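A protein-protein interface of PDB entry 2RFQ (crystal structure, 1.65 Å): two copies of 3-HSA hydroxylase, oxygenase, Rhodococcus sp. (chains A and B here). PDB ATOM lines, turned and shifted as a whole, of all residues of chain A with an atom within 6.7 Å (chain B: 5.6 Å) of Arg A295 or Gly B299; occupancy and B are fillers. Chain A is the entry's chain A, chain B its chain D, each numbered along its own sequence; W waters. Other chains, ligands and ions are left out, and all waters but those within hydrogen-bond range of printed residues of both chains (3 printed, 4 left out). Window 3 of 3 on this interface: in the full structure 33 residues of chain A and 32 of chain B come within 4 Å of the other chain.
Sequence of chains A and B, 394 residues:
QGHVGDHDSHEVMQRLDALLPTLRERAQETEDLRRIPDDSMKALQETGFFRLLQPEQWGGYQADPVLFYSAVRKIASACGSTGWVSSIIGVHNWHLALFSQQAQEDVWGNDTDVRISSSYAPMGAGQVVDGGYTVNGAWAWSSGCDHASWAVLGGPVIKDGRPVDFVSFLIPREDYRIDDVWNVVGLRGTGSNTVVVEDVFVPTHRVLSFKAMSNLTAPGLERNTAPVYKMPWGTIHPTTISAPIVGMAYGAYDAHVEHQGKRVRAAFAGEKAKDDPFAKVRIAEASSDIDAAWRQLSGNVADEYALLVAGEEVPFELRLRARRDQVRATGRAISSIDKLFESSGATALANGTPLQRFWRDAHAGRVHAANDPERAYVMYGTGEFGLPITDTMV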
ATOM      1  N   TYR A 250      17.912  19.415 -17.826  1.00  0.00           N
ATOM      2  CA  TYR A 250      17.313  18.377 -18.688  1.00  0.00           C
ATOM      3  C   TYR A 250      18.281  17.203 -18.873  1.00  0.00           C
ATOM      4  O   TYR A 250      17.894  16.013 -18.771  1.00  0.00           O
ATOM      5  CB  TYR A 250      16.908  18.934 -20.054  1.00  0.00           C
ATOM      6  CG  TYR A 250      15.554  19.618 -20.069  1.00  0.00           C
ATOM      7  CD1 TYR A 250      15.447  20.968 -19.785  1.00  0.00           C
ATOM      8  CD2 TYR A 250      14.390  18.898 -20.320  1.00  0.00           C
ATOM      9  CE1 TYR A 250      14.205  21.624 -19.821  1.00  0.00           C
ATOM     10  CE2 TYR A 250      13.128  19.533 -20.335  1.00  0.00           C
ATOM     11  CZ  TYR A 250      13.064  20.908 -20.066  1.00  0.00           C
ATOM     12  OH  TYR A 250      11.849  21.560 -20.073  1.00  0.00           O
ATOM     13  N   ILE A 290      11.888  21.581 -13.442  1.00  0.00           N
ATOM     14  CA  ILE A 290      12.637  21.872 -14.673  1.00  0.00           C
ATOM     15  C   ILE A 290      11.654  22.341 -15.732  1.00  0.00           C
ATOM     16  O   ILE A 290      11.884  23.363 -16.385  1.00  0.00           O
ATOM     17  CB  ILE A 290      13.445  20.641 -15.155  1.00  0.00           C
ATOM     18  CG1 ILE A 290      14.566  20.349 -14.141  1.00  0.00           C
ATOM     19  CG2 ILE A 290      13.996  20.910 -16.555  1.00  0.00           C
ATOM     20  CD1 ILE A 290      15.126  18.918 -14.287  1.00  0.00           C
ATOM     21  N   ASP A 291      10.533  21.627 -15.876  1.00  0.00           N
ATOM     22  CA  ASP A 291       9.551  22.018 -16.876  1.00  0.00           C
ATOM     23  C   ASP A 291       8.991  23.429 -16.569  1.00  0.00           C
ATOM     24  O   ASP A 291       8.799  24.259 -17.473  1.00  0.00           O
ATOM     25  CB  ASP A 291       8.409  21.008 -16.879  1.00  0.00           C
ATOM     26  CG  ASP A 291       7.314  21.400 -17.847  1.00  0.00           C
ATOM     27  OD1 ASP A 291       7.508  21.208 -19.074  1.00  0.00           O
ATOM     28  OD2 ASP A 291       6.275  21.930 -17.397  1.00  0.00           O
ATOM     29  N   ALA A 292       8.728  23.707 -15.291  1.00  0.00           N
ATOM     30  CA  ALA A 292       8.209  25.035 -14.927  1.00  0.00           C
ATOM     31  C   ALA A 292       9.213  26.131 -15.312  1.00  0.00           C
ATOM     32  O   ALA A 292       8.839  27.183 -15.855  1.00  0.00           O
ATOM     33  CB  ALA A 292       7.902  25.097 -13.439  1.00  0.00           C
ATOM     34  N   ALA A 293      10.486  25.872 -15.013  1.00  0.00           N
ATOM     35  CA  ALA A 293      11.571  26.794 -15.372  1.00  0.00           C
ATOM     36  C   ALA A 293      11.534  27.098 -16.861  1.00  0.00           C
ATOM     37  O   ALA A 293      11.539  28.254 -17.254  1.00  0.00           O
ATOM     38  CB  ALA A 293      12.918  26.206 -14.985  1.00  0.00           C
ATOM     39  N   TRP A 294      11.491  26.062 -17.685  1.00  0.00           N
ATOM     40  CA  TRP A 294      11.446  26.255 -19.130  1.00  0.00           C
ATOM     41  C   TRP A 294      10.170  26.969 -19.608  1.00  0.00           C
ATOM     42  O   TRP A 294      10.236  27.865 -20.438  1.00  0.00           O
ATOM     43  CB  TRP A 294      11.618  24.919 -19.852  1.00  0.00           C
ATOM     44  CG  TRP A 294      11.600  25.112 -21.343  1.00  0.00           C
ATOM     45  CD1 TRP A 294      10.609  24.728 -22.211  1.00  0.00           C
ATOM     46  CD2 TRP A 294      12.581  25.806 -22.130  1.00  0.00           C
ATOM     47  NE1 TRP A 294      10.927  25.126 -23.502  1.00  0.00           N
ATOM     48  CE2 TRP A 294      12.127  25.785 -23.477  1.00  0.00           C
ATOM     49  CE3 TRP A 294      13.803  26.443 -21.823  1.00  0.00           C
ATOM     50  CZ2 TRP A 294      12.858  26.367 -24.532  1.00  0.00           C
ATOM     51  CZ3 TRP A 294      14.542  27.018 -22.884  1.00  0.00           C
ATOM     52  CH2 TRP A 294      14.047  26.975 -24.218  1.00  0.00           C
ATOM     53  N   ARG A 295       9.018  26.581 -19.066  1.00  0.00           N
ATOM     54  CA  ARG A 295       7.749  27.229 -19.457  1.00  0.00           C
ATOM     55  C   ARG A 295       7.800  28.721 -19.217  1.00  0.00           C
ATOM     56  O   ARG A 295       7.410  29.493 -20.082  1.00  0.00           O
ATOM     57  CB  ARG A 295       6.583  26.628 -18.698  1.00  0.00           C
ATOM     58  CG  ARG A 295       6.123  25.284 -19.261  1.00  0.00           C
ATOM     59  CD  ARG A 295       4.877  24.851 -18.517  1.00  0.00           C
ATOM     60  NE  ARG A 295       4.484  23.472 -18.825  1.00  0.00           N
ATOM     61  CZ  ARG A 295       3.704  23.137 -19.856  1.00  0.00           C
ATOM     62  NH1 ARG A 295       3.199  24.067 -20.672  1.00  0.00           N
ATOM     63  NH2 ARG A 295       3.418  21.862 -20.083  1.00  0.00           N
ATOM     64  N   GLN A 296       8.313  29.126 -18.054  1.00  0.00           N
ATOM     65  CA  GLN A 296       8.402  30.577 -17.777  1.00  0.00           C
ATOM     66  C   GLN A 296       9.492  31.263 -18.595  1.00  0.00           C
ATOM     67  O   GLN A 296       9.273  32.351 -19.169  1.00  0.00           O
ATOM     68  CB  GLN A 296       8.634  30.809 -16.287  1.00  0.00           C
ATOM     69  CG  GLN A 296       7.447  30.305 -15.476  1.00  0.00           C
ATOM     70  CD  GLN A 296       7.520  30.700 -14.022  1.00  0.00           C
ATOM     71  OE1 GLN A 296       8.506  30.399 -13.329  1.00  0.00           O
ATOM     72  NE2 GLN A 296       6.468  31.393 -13.542  1.00  0.00           N
ATOM     73  N   LEU A 297      10.668  30.641 -18.656  1.00  0.00           N
ATOM     74  CA  LEU A 297      11.784  31.258 -19.361  1.00  0.00           C
ATOM     75  C   LEU A 297      11.478  31.458 -20.841  1.00  0.00           C
ATOM     76  O   LEU A 297      11.669  32.546 -21.380  1.00  0.00           O
ATOM     77  CB  LEU A 297      13.057  30.413 -19.184  1.00  0.00           C
ATOM     78  CG  LEU A 297      14.340  31.107 -19.639  1.00  0.00           C
ATOM     79  CD1 LEU A 297      14.772  32.195 -18.622  1.00  0.00           C
ATOM     80  CD2 LEU A 297      15.414  30.068 -19.763  1.00  0.00           C
ATOM     81  N   SER A 298      10.990  30.405 -21.490  1.00  0.00           N
ATOM     82  CA  SER A 298      10.609  30.511 -22.888  1.00  0.00           C
ATOM     83  C   SER A 298       9.307  31.317 -23.070  1.00  0.00           C
ATOM     84  O   SER A 298       9.158  32.078 -24.053  1.00  0.00           O
ATOM     85  CB  SER A 298      10.530  29.119 -23.504  1.00  0.00           C
ATOM     86  OG  SER A 298       9.442  28.367 -23.005  1.00  0.00           O
ATOM     87  N   GLY A 299       8.382  31.184 -22.110  1.00  0.00           N
ATOM     88  CA  GLY A 299       7.082  31.890 -22.149  1.00  0.00           C
ATOM     89  C   GLY A 299       7.205  33.401 -22.165  1.00  0.00           C
ATOM     90  O   GLY A 299       6.537  34.087 -22.968  1.00  0.00           O
ATOM     91  N   ASN A 300       8.018  33.940 -21.259  1.00  0.00           N
ATOM     92  CA  ASN A 300       8.196  35.381 -21.214  1.00  0.00           C
ATOM     93  C   ASN A 300       8.861  35.891 -22.498  1.00  0.00           C
ATOM     94  O   ASN A 300       8.487  36.932 -23.015  1.00  0.00           O
ATOM     95  CB  ASN A 300       9.005  35.780 -19.975  1.00  0.00           C
ATOM     96  CG  ASN A 300       8.250  35.563 -18.687  1.00  0.00           C
ATOM     97  OD1 ASN A 300       8.842  35.107 -17.674  1.00  0.00           O
ATOM     98  ND2 ASN A 300       6.967  35.911 -18.673  1.00  0.00           N
ATOM     99  N   TRP B 294      -0.082  27.838 -12.658  1.00  0.00           N
ATOM    100  CA  TRP B 294      -1.097  27.996 -13.696  1.00  0.00           C
ATOM    101  C   TRP B 294      -0.594  27.580 -15.077  1.00  0.00           C
ATOM    102  O   TRP B 294      -1.296  26.919 -15.820  1.00  0.00           O
ATOM    103  CB  TRP B 294      -1.624  29.428 -13.732  1.00  0.00           C
ATOM    104  CG  TRP B 294      -2.665  29.594 -14.797  1.00  0.00           C
ATOM    105  CD1 TRP B 294      -2.543  30.296 -15.958  1.00  0.00           C
ATOM    106  CD2 TRP B 294      -3.989  29.035 -14.796  1.00  0.00           C
ATOM    107  NE1 TRP B 294      -3.718  30.218 -16.693  1.00  0.00           N
ATOM    108  CE2 TRP B 294      -4.616  29.444 -16.004  1.00  0.00           C
ATOM    109  CE3 TRP B 294      -4.697  28.202 -13.908  1.00  0.00           C
ATOM    110  CZ2 TRP B 294      -5.927  29.052 -16.347  1.00  0.00           C
ATOM    111  CZ3 TRP B 294      -6.017  27.824 -14.254  1.00  0.00           C
ATOM    112  CH2 TRP B 294      -6.603  28.253 -15.455  1.00  0.00           C
ATOM    113  N   ARG B 295       0.635  27.942 -15.426  1.00  0.00           N
ATOM    114  CA  ARG B 295       1.160  27.522 -16.737  1.00  0.00           C
ATOM    115  C   ARG B 295       1.137  26.013 -16.923  1.00  0.00           C
ATOM    116  O   ARG B 295       0.746  25.535 -17.988  1.00  0.00           O
ATOM    117  CB  ARG B 295       2.584  28.011 -16.923  1.00  0.00           C
ATOM    118  CG  ARG B 295       2.659  29.507 -17.154  1.00  0.00           C
ATOM    119  CD  ARG B 295       4.099  29.904 -17.486  1.00  0.00           C
ATOM    120  NE  ARG B 295       4.256  31.358 -17.662  1.00  0.00           N
ATOM    121  CZ  ARG B 295       4.218  31.979 -18.845  1.00  0.00           C
ATOM    122  NH1 ARG B 295       3.998  31.308 -19.971  1.00  0.00           N
ATOM    123  NH2 ARG B 295       4.391  33.298 -18.905  1.00  0.00           N
ATOM    124  N   GLN B 296       1.544  25.278 -15.891  1.00  0.00           N
ATOM    125  CA  GLN B 296       1.562  23.813 -16.002  1.00  0.00           C
ATOM    126  C   GLN B 296       0.150  23.241 -15.964  1.00  0.00           C
ATOM    127  O   GLN B 296      -0.193  22.376 -16.791  1.00  0.00           O
ATOM    128  CB  GLN B 296       2.408  23.198 -14.897  1.00  0.00           C
ATOM    129  CG  GLN B 296       3.881  23.589 -15.041  1.00  0.00           C
ATOM    130  CD  GLN B 296       4.761  22.833 -14.086  1.00  0.00           C
ATOM    131  OE1 GLN B 296       4.542  22.862 -12.870  1.00  0.00           O
ATOM    132  NE2 GLN B 296       5.775  22.160 -14.625  1.00  0.00           N
ATOM    133  N   LEU B 297      -0.666  23.709 -15.016  1.00  0.00           N
ATOM    134  CA  LEU B 297      -2.010  23.163 -14.877  1.00  0.00           C
ATOM    135  C   LEU B 297      -2.816  23.354 -16.187  1.00  0.00           C
ATOM    136  O   LEU B 297      -3.428  22.403 -16.714  1.00  0.00           O
ATOM    137  CB  LEU B 297      -2.723  23.806 -13.668  1.00  0.00           C
ATOM    138  CG  LEU B 297      -4.018  23.098 -13.275  1.00  0.00           C
ATOM    139  CD1 LEU B 297      -3.729  21.777 -12.560  1.00  0.00           C
ATOM    140  CD2 LEU B 297      -4.861  24.009 -12.394  1.00  0.00           C
ATOM    141  N   SER B 298      -2.823  24.593 -16.685  1.00  0.00           N
ATOM    142  CA  SER B 298      -3.543  24.922 -17.919  1.00  0.00           C
ATOM    143  C   SER B 298      -2.834  24.338 -19.135  1.00  0.00           C
ATOM    144  O   SER B 298      -3.492  23.892 -20.066  1.00  0.00           O
ATOM    145  CB  SER B 298      -3.784  26.441 -18.050  1.00  0.00           C
ATOM    146  OG  SER B 298      -2.573  27.138 -18.265  1.00  0.00           O
ATOM    147  N   GLY B 299      -1.496  24.287 -19.100  1.00  0.00           N
ATOM    148  CA  GLY B 299      -0.714  23.799 -20.230  1.00  0.00           C
ATOM    149  C   GLY B 299      -0.963  22.339 -20.527  1.00  0.00           C
ATOM    150  O   GLY B 299      -1.107  21.945 -21.687  1.00  0.00           O
ATOM    151  N   ASN B 300      -0.969  21.517 -19.482  1.00  0.00           N
ATOM    152  CA  ASN B 300      -1.225  20.102 -19.677  1.00  0.00           C
ATOM    153  C   ASN B 300      -2.633  19.856 -20.208  1.00  0.00           C
ATOM    154  O   ASN B 300      -2.819  19.042 -21.097  1.00  0.00           O
ATOM    155  CB  ASN B 300      -0.955  19.317 -18.383  1.00  0.00           C
ATOM    156  CG  ASN B 300       0.509  19.332 -17.986  1.00  0.00           C
ATOM    157  OD1 ASN B 300       0.851  19.432 -16.781  1.00  0.00           O
ATOM    158  ND2 ASN B 300       1.390  19.193 -18.974  1.00  0.00           N
ATOM    159  N   VAL B 301      -3.616  20.590 -19.684  1.00  0.00           N
ATOM    160  CA  VAL B 301      -4.989  20.484 -20.196  1.00  0.00           C
ATOM    161  C   VAL B 301      -5.026  20.884 -21.670  1.00  0.00           C
ATOM    162  O   VAL B 301      -5.626  20.194 -22.502  1.00  0.00           O
ATOM    163  CB  VAL B 301      -5.953  21.365 -19.388  1.00  0.00           C
ATOM    164  CG1 VAL B 301      -7.314  21.464 -20.077  1.00  0.00           C
ATOM    165  CG2 VAL B 301      -6.099  20.807 -17.977  1.00  0.00           C
ATOM    166  N   ALA B 302      -4.369  21.998 -21.986  1.00  0.00           N
ATOM    167  CA  ALA B 302      -4.378  22.487 -23.363  1.00  0.00           C
ATOM    168  C   ALA B 302      -3.768  21.469 -24.318  1.00  0.00           C
ATOM    169  O   ALA B 302      -4.301  21.245 -25.424  1.00  0.00           O
ATOM    170  CB  ALA B 302      -3.687  23.841 -23.473  1.00  0.00           C
ATOM    171  N   ASP B 303      -2.672  20.842 -23.884  1.00  0.00           N
ATOM    172  CA  ASP B 303      -1.965  19.866 -24.723  1.00  0.00           C
ATOM    173  C   ASP B 303      -2.818  18.644 -24.990  1.00  0.00           C
ATOM    174  O   ASP B 303      -2.904  18.158 -26.129  1.00  0.00           O
ATOM    175  CB  ASP B 303      -0.632  19.476 -24.095  1.00  0.00           C
ATOM    176  CG  ASP B 303       0.413  20.568 -24.216  1.00  0.00           C
ATOM    177  OD1 ASP B 303       0.133  21.617 -24.849  1.00  0.00           O
ATOM    178  OD2 ASP B 303       1.516  20.346 -23.703  1.00  0.00           O
ATOM    179  N   GLU B 304      -3.462  18.138 -23.944  1.00  0.00           N
ATOM    180  CA  GLU B 304      -4.388  17.015 -24.117  1.00  0.00           C
ATOM    181  C   GLU B 304      -5.502  17.368 -25.098  1.00  0.00           C
ATOM    182  O   GLU B 304      -5.821  16.611 -26.024  1.00  0.00           O
ATOM    183  CB  GLU B 304      -4.984  16.625 -22.767  1.00  0.00           C
ATOM    184  CG  GLU B 304      -3.955  16.052 -21.803  1.00  0.00           C
ATOM    185  CD  GLU B 304      -4.559  15.580 -20.484  1.00  0.00           C
ATOM    186  OE1 GLU B 304      -5.785  15.706 -20.293  1.00  0.00           O
ATOM    187  OE2 GLU B 304      -3.782  15.102 -19.623  1.00  0.00           O
ATOM    188  N   ARG B 321       2.326  13.271 -16.687  1.00  0.00           N
ATOM    189  CA  ARG B 321       2.817  14.641 -16.462  1.00  0.00           C
ATOM    190  C   ARG B 321       1.699  15.524 -15.882  1.00  0.00           C
ATOM    191  O   ARG B 321       1.932  16.330 -14.987  1.00  0.00           O
ATOM    192  CB  ARG B 321       3.373  15.240 -17.752  1.00  0.00           C
ATOM    193  CG  ARG B 321       4.746  14.698 -18.089  1.00  0.00           C
ATOM    194  CD  ARG B 321       5.407  15.514 -19.180  1.00  0.00           C
ATOM    195  NE  ARG B 321       4.821  15.244 -20.488  1.00  0.00           N
ATOM    196  CZ  ARG B 321       4.258  16.150 -21.274  1.00  0.00           C
ATOM    197  NH1 ARG B 321       4.169  17.427 -20.887  1.00  0.00           N
ATOM    198  NH2 ARG B 321       3.788  15.766 -22.461  1.00  0.00           N
ATOM    199  N   ASP B 325       2.136  17.545 -12.360  1.00  0.00           N
ATOM    200  CA  ASP B 325       2.093  19.002 -12.232  1.00  0.00           C
ATOM    201  C   ASP B 325       0.868  19.540 -11.531  1.00  0.00           C
ATOM    202  O   ASP B 325       0.884  20.663 -11.021  1.00  0.00           O
ATOM    203  CB  ASP B 325       2.174  19.650 -13.623  1.00  0.00           C
ATOM    204  CG  ASP B 325       3.502  19.352 -14.322  1.00  0.00           C
ATOM    205  OD1 ASP B 325       4.523  19.074 -13.631  1.00  0.00           O
ATOM    206  OD2 ASP B 325       3.528  19.406 -15.567  1.00  0.00           O
HETATM  207  O   HOH W   1       3.660  32.377 -22.687  1.00  0.00           O
HETATM  208  O   HOH W   2       4.430  36.155 -19.609  1.00  0.00           O
HETATM  209  O   HOH W   3       5.547  35.036 -16.603  1.00  0.00           O
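Arg A295 touches Arg B295 (O to NH1, 3.9 Å).
Arg A295 touches Gln B296.
Arg A295 touches Gly B299.
ND2 of Asn B300 touches NH2 of Arg A295, 3.5 Å away.
CG of Gln A296 touches CD of Arg B295, 3.9 Å away.
CA of Gly A299 touches NH1 of Arg B295 (3.8 Å).
ND2 of Asn A300 touches NH2 of Arg B295, at 3.7 Å.
Arg A295 touches its own counterpart, Arg B295.
Arg A295 touches Gln B296, and with the chains exchanged Gln A296 touches Arg B295.
Arg A295 touches Gly B299, and with the chains exchanged Gly A299 touches Arg B295.
Arg A295 touches Asn B300, and with the chains exchanged Asn A300 touches Arg B295.
Positions printed for both chains: 294, 295, 296, 297, 298, 299 and 300.
Of the 9 pairs that touch across the chains among the printed residues, 7 have their exchanged pair printed and touching as well.
Tyr A250 touches none of the printed residues of chain B.
Printed residues of chain B within 4 Å of Ala A292: Gln B296 (3.4 Å).
Arg A295 touches just these residues of chain B: Arg B295, Gln B296, Gly B299 and Asn B300.
Of the printed residues of chain B, Gln A296 touches Arg B295 (3.9 Å).
Of the printed residues of chain B, Asn A300 touches Arg B295.
Of the printed residues of chain A, Gln B296 touches Asp A291, Ala A292 and Arg A295.
Gly B299 touches just one residue of chain A: Arg A295 (3.9 Å).
Printed residues of chain A within 4 Å of Asn B300: Arg A295 (3.5 Å).
Ala B302 touches none of the printed residues of chain A.
The nearest printed residue of chain A that does not touch Gly B299 is Asp A291 (7.8 Å).
The nearest printed residue of chain A that does not touch Asn B300 is Asp A291 (5.8 Å).
Water W3 lies within hydrogen-bond range of ND2 of Asn A300 (2.7 Å) and NH2 of Arg B295 (3.1 Å).
Water W2 lies within hydrogen-bond range of the side-chain amide nitrogen (ND2) of Asn A300 (2.7 Å) and the guanidinium group (NH2) of Arg B295 (2.9 Å).
Water W1 lies within hydrogen-bond range of NH1 of Arg B295 (2.9 Å) and O of Gly A299 (3.4 Å).
NE of Arg A295 is in salt-bridge range of OD2 of Asp A291 (2.8 Å).
OD2 of Asp B325 sits close to OD1 of Asn B300.
The side-chain amide nitrogen of Gln B296 lies within hydrogen-bond range of the side-chain carboxylate of Asp B325.
OD1 of Asn B300 lies close to O of Gln B296.
OD1 of Asn A300 sits close to O of Gln A296, 3.2 Å away.
Among the printed residues, no Asp or Glu carboxylate lies within 4 Å of a Lys or Arg side-chain nitrogen of the other chain.
N of Ala A292 sits close to NE2 of Gln B296 (3.4 Å).
The side-chain amide nitrogen (NE2) of Gln B296 lies within hydrogen-bond range of the side-chain carboxylate (OD2) of Asp A291 (2.8 Å).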
